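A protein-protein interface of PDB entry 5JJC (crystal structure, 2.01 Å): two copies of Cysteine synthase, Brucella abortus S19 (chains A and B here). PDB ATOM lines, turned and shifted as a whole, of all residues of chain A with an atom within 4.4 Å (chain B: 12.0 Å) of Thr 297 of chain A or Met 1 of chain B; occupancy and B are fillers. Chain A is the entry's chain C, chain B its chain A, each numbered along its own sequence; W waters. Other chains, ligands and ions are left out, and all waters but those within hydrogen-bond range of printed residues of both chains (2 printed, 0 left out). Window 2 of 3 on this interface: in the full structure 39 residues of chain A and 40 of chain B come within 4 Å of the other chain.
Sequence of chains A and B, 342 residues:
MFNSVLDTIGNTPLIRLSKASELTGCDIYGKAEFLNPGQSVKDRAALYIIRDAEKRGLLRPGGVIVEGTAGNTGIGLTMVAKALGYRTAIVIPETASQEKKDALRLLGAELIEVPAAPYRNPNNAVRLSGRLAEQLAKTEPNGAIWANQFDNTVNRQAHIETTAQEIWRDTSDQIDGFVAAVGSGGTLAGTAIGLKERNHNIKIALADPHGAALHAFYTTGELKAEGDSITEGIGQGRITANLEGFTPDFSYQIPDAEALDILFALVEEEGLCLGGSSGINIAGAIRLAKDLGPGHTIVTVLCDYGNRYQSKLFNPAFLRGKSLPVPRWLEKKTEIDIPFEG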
ATOM      1  N   LEU A  14      12.533  -0.348  34.845  1.00  0.00           N
ATOM      2  CA  LEU A  14      13.472  -1.000  33.938  1.00  0.00           C
ATOM      3  C   LEU A  14      14.831  -0.322  34.045  1.00  0.00           C
ATOM      4  O   LEU A  14      14.935   0.895  33.903  1.00  0.00           O
ATOM      5  CB  LEU A  14      12.969  -0.932  32.485  1.00  0.00           C
ATOM      6  CG  LEU A  14      11.625  -1.622  32.223  1.00  0.00           C
ATOM      7  CD1 LEU A  14      11.221  -1.502  30.758  1.00  0.00           C
ATOM      8  CD2 LEU A  14      11.676  -3.094  32.654  1.00  0.00           C
ATOM      9  N   ASP A  27      19.152  -2.751  23.073  1.00  0.00           N
ATOM     10  CA  ASP A  27      18.835  -2.131  24.357  1.00  0.00           C
ATOM     11  C   ASP A  27      18.260  -3.205  25.274  1.00  0.00           C
ATOM     12  O   ASP A  27      17.113  -3.613  25.128  1.00  0.00           O
ATOM     13  CB  ASP A  27      17.855  -0.972  24.213  1.00  0.00           C
ATOM     14  CG  ASP A  27      18.509   0.274  23.638  1.00  0.00           C
ATOM     15  OD1 ASP A  27      19.623   0.632  24.072  1.00  0.00           O
ATOM     16  OD2 ASP A  27      17.916   0.880  22.733  1.00  0.00           O
ATOM     17  N   TYR A  29      17.216  -4.380  29.057  1.00  0.00           N
ATOM     18  CA  TYR A  29      16.794  -3.852  30.348  1.00  0.00           C
ATOM     19  C   TYR A  29      16.473  -4.970  31.334  1.00  0.00           C
ATOM     20  O   TYR A  29      15.939  -6.006  30.952  1.00  0.00           O
ATOM     21  CB  TYR A  29      15.562  -2.950  30.194  1.00  0.00           C
ATOM     22  CG  TYR A  29      15.810  -1.711  29.372  1.00  0.00           C
ATOM     23  CD1 TYR A  29      16.212  -0.522  29.971  1.00  0.00           C
ATOM     24  CD2 TYR A  29      15.636  -1.726  28.000  1.00  0.00           C
ATOM     25  CE1 TYR A  29      16.446   0.618  29.212  1.00  0.00           C
ATOM     26  CE2 TYR A  29      15.873  -0.599  27.238  1.00  0.00           C
ATOM     27  CZ  TYR A  29      16.270   0.570  27.847  1.00  0.00           C
ATOM     28  OH  TYR A  29      16.499   1.687  27.077  1.00  0.00           O
ATOM     29  N   ASP A 170       6.230   0.774  29.895  1.00  0.00           N
ATOM     30  CA  ASP A 170       7.518   1.411  30.129  1.00  0.00           C
ATOM     31  C   ASP A 170       8.462   1.324  28.938  1.00  0.00           C
ATOM     32  O   ASP A 170       9.417   2.105  28.853  1.00  0.00           O
ATOM     33  CB  ASP A 170       8.181   0.819  31.369  1.00  0.00           C
ATOM     34  CG  ASP A 170       7.426   1.154  32.639  1.00  0.00           C
ATOM     35  OD1 ASP A 170       6.547   2.048  32.596  1.00  0.00           O
ATOM     36  OD2 ASP A 170       7.715   0.526  33.679  1.00  0.00           O
ATOM     37  N   THR A 171       8.211   0.402  28.014  1.00  0.00           N
ATOM     38  CA  THR A 171       8.990   0.388  26.781  1.00  0.00           C
ATOM     39  C   THR A 171       8.271   1.166  25.675  1.00  0.00           C
ATOM     40  O   THR A 171       8.730   1.188  24.535  1.00  0.00           O
ATOM     41  CB  THR A 171       9.287  -1.045  26.278  1.00  0.00           C
ATOM     42  OG1 THR A 171       8.059  -1.746  26.052  1.00  0.00           O
ATOM     43  CG2 THR A 171      10.141  -1.811  27.290  1.00  0.00           C
ATOM     44  N   GLN A 174       7.696  -0.704  22.534  1.00  0.00           N
ATOM     45  CA  GLN A 174       8.829  -1.102  21.685  1.00  0.00           C
ATOM     46  C   GLN A 174       9.540  -2.424  22.017  1.00  0.00           C
ATOM     47  O   GLN A 174      10.435  -2.845  21.263  1.00  0.00           O
ATOM     48  CB  GLN A 174       9.874   0.023  21.657  1.00  0.00           C
ATOM     49  CG  GLN A 174       9.258   1.367  21.355  1.00  0.00           C
ATOM     50  CD  GLN A 174       9.100   1.612  19.877  1.00  0.00           C
ATOM     51  OE1 GLN A 174       8.400   0.881  19.202  1.00  0.00           O
ATOM     52  NE2 GLN A 174       9.711   2.660  19.371  1.00  0.00           N
ATOM     53  N   ILE A 175       9.139  -3.103  23.087  1.00  0.00           N
ATOM     54  CA  ILE A 175       9.799  -4.361  23.438  1.00  0.00           C
ATOM     55  C   ILE A 175       9.700  -5.426  22.323  1.00  0.00           C
ATOM     56  O   ILE A 175       8.629  -5.670  21.755  1.00  0.00           O
ATOM     57  CB  ILE A 175       9.242  -4.935  24.767  1.00  0.00           C
ATOM     58  CG1 ILE A 175       9.913  -6.280  25.081  1.00  0.00           C
ATOM     59  CG2 ILE A 175       7.703  -5.041  24.755  1.00  0.00           C
ATOM     60  CD1 ILE A 175       9.527  -6.879  26.402  1.00  0.00           C
ATOM     61  N   ASP A 176      10.838  -6.043  22.002  1.00  0.00           N
ATOM     62  CA  ASP A 176      10.911  -7.046  20.944  1.00  0.00           C
ATOM     63  C   ASP A 176      11.062  -8.448  21.492  1.00  0.00           C
ATOM     64  O   ASP A 176      10.661  -9.416  20.842  1.00  0.00           O
ATOM     65  CB  ASP A 176      12.080  -6.745  20.005  1.00  0.00           C
ATOM     66  CG  ASP A 176      11.920  -5.424  19.295  1.00  0.00           C
ATOM     67  OD1 ASP A 176      12.788  -4.547  19.477  1.00  0.00           O
ATOM     68  OD2 ASP A 176      10.915  -5.259  18.578  1.00  0.00           O
ATOM     69  N   GLY A 177      11.656  -8.555  22.673  1.00  0.00           N
ATOM     70  CA  GLY A 177      11.918  -9.852  23.274  1.00  0.00           C
ATOM     71  C   GLY A 177      11.888  -9.829  24.792  1.00  0.00           C
ATOM     72  O   GLY A 177      12.264  -8.833  25.404  1.00  0.00           O
ATOM     73  N   HIS A 296      17.323  -4.189  18.686  1.00  0.00           N
ATOM     74  CA  HIS A 296      16.109  -4.663  19.347  1.00  0.00           C
ATOM     75  C   HIS A 296      16.084  -4.281  20.816  1.00  0.00           C
ATOM     76  O   HIS A 296      17.121  -4.022  21.416  1.00  0.00           O
ATOM     77  CB  HIS A 296      15.977  -6.183  19.224  1.00  0.00           C
ATOM     78  CG  HIS A 296      15.685  -6.642  17.823  1.00  0.00           C
ATOM     79  ND1 HIS A 296      16.670  -7.024  16.960  1.00  0.00           N
ATOM     80  CD2 HIS A 296      14.509  -6.742  17.157  1.00  0.00           C
ATOM     81  CE1 HIS A 296      16.116  -7.370  15.796  1.00  0.00           C
ATOM     82  NE2 HIS A 296      14.820  -7.206  15.894  1.00  0.00           N
ATOM     83  N   THR A 297      14.886  -4.264  21.383  1.00  0.00           N
ATOM     84  CA  THR A 297      14.712  -4.006  22.798  1.00  0.00           C
ATOM     85  C   THR A 297      14.357  -5.316  23.506  1.00  0.00           C
ATOM     86  O   THR A 297      13.344  -5.937  23.189  1.00  0.00           O
ATOM     87  CB  THR A 297      13.619  -2.965  23.038  1.00  0.00           C
ATOM     88  OG1 THR A 297      13.973  -1.735  22.388  1.00  0.00           O
ATOM     89  CG2 THR A 297      13.442  -2.717  24.526  1.00  0.00           C
ATOM     90  N   ILE A 298      15.198  -5.726  24.457  1.00  0.00           N
ATOM     91  CA  ILE A 298      15.046  -6.997  25.181  1.00  0.00           C
ATOM     92  C   ILE A 298      14.828  -6.710  26.668  1.00  0.00           C
ATOM     93  O   ILE A 298      15.542  -5.897  27.244  1.00  0.00           O
ATOM     94  CB  ILE A 298      16.315  -7.906  25.034  1.00  0.00           C
ATOM     95  CG1 ILE A 298      16.707  -8.107  23.563  1.00  0.00           C
ATOM     96  CG2 ILE A 298      16.133  -9.251  25.753  1.00  0.00           C
ATOM     97  CD1 ILE A 298      15.665  -8.789  22.749  1.00  0.00           C
ATOM     98  N   VAL A 299      13.859  -7.366  27.300  1.00  0.00           N
ATOM     99  CA  VAL A 299      13.656  -7.160  28.728  1.00  0.00           C
ATOM    100  C   VAL A 299      13.764  -8.492  29.451  1.00  0.00           C
ATOM    101  O   VAL A 299      13.334  -9.524  28.932  1.00  0.00           O
ATOM    102  CB  VAL A 299      12.289  -6.490  29.016  1.00  0.00           C
ATOM    103  CG1 VAL A 299      11.977  -6.484  30.509  1.00  0.00           C
ATOM    104  CG2 VAL A 299      12.259  -5.052  28.423  1.00  0.00           C
ATOM    105  N   MET B   1      12.154   2.986  31.274  1.00  0.00           N
ATOM    106  CA  MET B   1      13.430   2.767  30.611  1.00  0.00           C
ATOM    107  C   MET B   1      14.486   3.703  31.192  1.00  0.00           C
ATOM    108  O   MET B   1      14.656   4.842  30.746  1.00  0.00           O
ATOM    109  CB  MET B   1      13.286   2.956  29.100  1.00  0.00           C
ATOM    110  CG  MET B   1      12.774   1.701  28.395  1.00  0.00           C
ATOM    111  SD  MET B   1      12.321   1.974  26.673  1.00  0.00           S
ATOM    112  CE  MET B   1      13.331   0.805  25.803  1.00  0.00           C
ATOM    113  N   PHE B   2      15.178   3.215  32.216  1.00  0.00           N
ATOM    114  CA  PHE B   2      16.226   3.984  32.881  1.00  0.00           C
ATOM    115  C   PHE B   2      17.644   3.531  32.530  1.00  0.00           C
ATOM    116  O   PHE B   2      17.882   2.324  32.318  1.00  0.00           O
ATOM    117  CB  PHE B   2      16.051   3.910  34.405  1.00  0.00           C
ATOM    118  CG  PHE B   2      14.774   4.495  34.908  1.00  0.00           C
ATOM    119  CD1 PHE B   2      14.337   4.170  36.173  1.00  0.00           C
ATOM    120  CD2 PHE B   2      14.018   5.375  34.136  1.00  0.00           C
ATOM    121  CE1 PHE B   2      13.174   4.696  36.681  1.00  0.00           C
ATOM    122  CE2 PHE B   2      12.840   5.908  34.636  1.00  0.00           C
ATOM    123  CZ  PHE B   2      12.420   5.566  35.906  1.00  0.00           C
ATOM    124  N   ASN B   3      18.544   4.536  32.514  1.00  0.00           N
ATOM    125  CA  ASN B   3      19.974   4.429  32.172  1.00  0.00           C
ATOM    126  C   ASN B   3      20.945   3.690  33.096  1.00  0.00           C
ATOM    127  O   ASN B   3      21.915   3.041  32.603  1.00  0.00           O
ATOM    128  CB  ASN B   3      20.516   5.841  31.852  1.00  0.00           C
ATOM    129  CG  ASN B   3      20.749   6.024  30.337  1.00  0.00           C
ATOM    130  OD1 ASN B   3      21.060   7.135  29.911  1.00  0.00           O
ATOM    131  ND2 ASN B   3      20.836   4.931  29.605  1.00  0.00           N
ATOM    132  N   SER B   4      20.729   3.798  34.399  1.00  0.00           N
ATOM    133  CA  SER B   4      21.468   2.955  35.319  1.00  0.00           C
ATOM    134  C   SER B   4      20.651   2.848  36.590  1.00  0.00           C
ATOM    135  O   SER B   4      19.585   3.430  36.719  1.00  0.00           O
ATOM    136  CB  SER B   4      22.891   3.479  35.653  1.00  0.00           C
ATOM    137  OG  SER B   4      22.861   4.455  36.711  1.00  0.00           O
ATOM    138  N   VAL B   5      21.167   2.111  37.565  1.00  0.00           N
ATOM    139  CA  VAL B   5      20.461   1.894  38.854  1.00  0.00           C
ATOM    140  C   VAL B   5      20.304   3.235  39.582  1.00  0.00           C
ATOM    141  O   VAL B   5      19.421   3.412  40.411  1.00  0.00           O
ATOM    142  CB  VAL B   5      21.210   0.869  39.746  1.00  0.00           C
ATOM    143  CG1 VAL B   5      22.584   1.407  40.128  1.00  0.00           C
ATOM    144  CG2 VAL B   5      20.387   0.509  40.950  1.00  0.00           C
ATOM    145  N   LEU B   6      21.127   4.213  39.218  1.00  0.00           N
ATOM    146  CA  LEU B   6      21.057   5.509  39.890  1.00  0.00           C
ATOM    147  C   LEU B   6      19.728   6.212  39.602  1.00  0.00           C
ATOM    148  O   LEU B   6      19.270   7.027  40.400  1.00  0.00           O
ATOM    149  CB  LEU B   6      22.223   6.406  39.469  1.00  0.00           C
ATOM    150  CG  LEU B   6      23.647   5.873  39.687  1.00  0.00           C
ATOM    151  CD1 LEU B   6      24.662   6.949  39.315  1.00  0.00           C
ATOM    152  CD2 LEU B   6      23.869   5.427  41.106  1.00  0.00           C
ATOM    153  N   ASP B   7      19.119   5.919  38.456  1.00  0.00           N
ATOM    154  CA  ASP B   7      17.817   6.507  38.127  1.00  0.00           C
ATOM    155  C   ASP B   7      16.684   6.012  39.053  1.00  0.00           C
ATOM    156  O   ASP B   7      15.590   6.580  39.060  1.00  0.00           O
ATOM    157  CB  ASP B   7      17.449   6.213  36.669  1.00  0.00           C
ATOM    158  CG  ASP B   7      18.392   6.887  35.672  1.00  0.00           C
ATOM    159  OD1 ASP B   7      18.794   8.038  35.920  1.00  0.00           O
ATOM    160  OD2 ASP B   7      18.728   6.263  34.647  1.00  0.00           O
ATOM    161  N   THR B   8      16.934   4.958  39.827  1.00  0.00           N
ATOM    162  CA  THR B   8      15.889   4.419  40.698  1.00  0.00           C
ATOM    163  C   THR B   8      16.020   4.971  42.123  1.00  0.00           C
ATOM    164  O   THR B   8      15.223   4.639  43.000  1.00  0.00           O
ATOM    165  CB  THR B   8      15.898   2.860  40.736  1.00  0.00           C
ATOM    166  OG1 THR B   8      17.032   2.394  41.471  1.00  0.00           O
ATOM    167  CG2 THR B   8      15.940   2.285  39.328  1.00  0.00           C
ATOM    168  N   ILE B   9      17.019   5.826  42.348  1.00  0.00           N
ATOM    169  CA  ILE B   9      17.172   6.501  43.638  1.00  0.00           C
ATOM    170  C   ILE B   9      16.062   7.550  43.813  1.00  0.00           C
ATOM    171  O   ILE B   9      15.773   8.313  42.892  1.00  0.00           O
ATOM    172  CB  ILE B   9      18.573   7.167  43.753  1.00  0.00           C
ATOM    173  CG1 ILE B   9      19.677   6.094  43.757  1.00  0.00           C
ATOM    174  CG2 ILE B   9      18.682   8.053  44.993  1.00  0.00           C
ATOM    175  CD1 ILE B   9      21.079   6.679  43.669  1.00  0.00           C
HETATM  176  O   HOH W   1       9.770   4.390  27.615  1.00  0.00           O
HETATM  177  O   HOH W   2      11.120   1.828  34.030  1.00  0.00           O
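The backbone NH of Phe 2 of chain B lies within hydrogen-bond range of the backbone carbonyl oxygen of Leu 14 of chain A. The side-chain sulfur of Met 1 of chain B lies close to the backbone carbonyl oxygen of Asp 170 of chain A, 3.6 Å away.
N of Tyr 29 of chain A sits at hydrogen-bond distance from O of Ile 298 of chain A, 2.9 Å away. The side-chain hydroxyl (OG1) of Thr 171 of chain A lies within hydrogen-bond range of the backbone NH (N) of Ile 175 of chain A (3.4 Å). N of Gly 177 of chain A sits at hydrogen-bond distance from O of Thr 297 of chain A (3.2 Å). The backbone carbonyl oxygen (O) of Thr 297 of chain A sits at hydrogen-bond distance from the backbone NH (N) of Asp 176 of chain A (2.8 Å).
Among the printed residues, pairs that only touch across the chains: Tyr 29 of chain A with Met 1 of chain B (3.2 Å), Thr 171 of chain A with Met 1 of chain B (3.7 Å), Thr 297 of chain A with Met 1 of chain B (3.7 Å), Tyr 29 of chain A with Phe 2 of chain B (3.8 Å) and Leu 14 of chain A with Met 1 of chain B (3.9 Å).
Of chain B, only Met 1 (3.7 Å) comes within 4 Å of Thr 297 of chain A. Met 1 of chain B touches just these residues of chain A: Leu 14 (3.9 Å), Tyr 29 (3.2 Å), Asp 170 (3.4 Å), Thr 171 (3.7 Å) and Thr 297 (3.7 Å). Leu 14 of chain A touches just these residues of chain B: Met 1 (3.9 Å) and Phe 2 (2.9 Å). Of chain B, only Met 1 (3.2 Å) and Phe 2 (3.8 Å) come within 4 Å of Tyr 29 of chain A. Of the printed residues of chain B, Asp 170 of chain A touches Met 1. No residue of chain B comes within 4 Å of Gln 174 of chain A. No residue of chain B comes within 4 Å of Ile 175 of chain A. Asp 176 of chain A touches none of the printed residues of chain B. No residue of chain B comes within 4 Å of Gly 177 of chain A. No residue of chain B comes within 4 Å of His 296 of chain A. No residue of chain B comes within 4 Å of Ile 298 of chain A. Val 299 of chain A touches none of the printed residues of chain B. Printed residues of chain A within 4 Å of Phe 2 of chain B: Leu 14 and Tyr 29. Leu 6 of chain B touches none of the printed residues of chain A. The nearest printed residue of chain A that does not touch Met 1 of chain B is Asp 27 of chain A (5.1 Å).
Hydrophobic or aromatic side chains of chain B within 4 Å of the printed part of chain A: Met 1 and Phe 2. Along chain B the printed residues that touch a printed residue of chain A span positions 1 to 2.
No position is printed for both chains.
Water W1 bridges the backbone carbonyl oxygen (O) of Asp 170 of chain A (2.6 Å) and the side-chain sulfur (SD) of Met 1 of chain B (3.6 Å). Water W2 lies within hydrogen-bond range of N of Leu 14 of chain A (2.7 Å) and N of Met 1 of chain B (3.2 Å).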
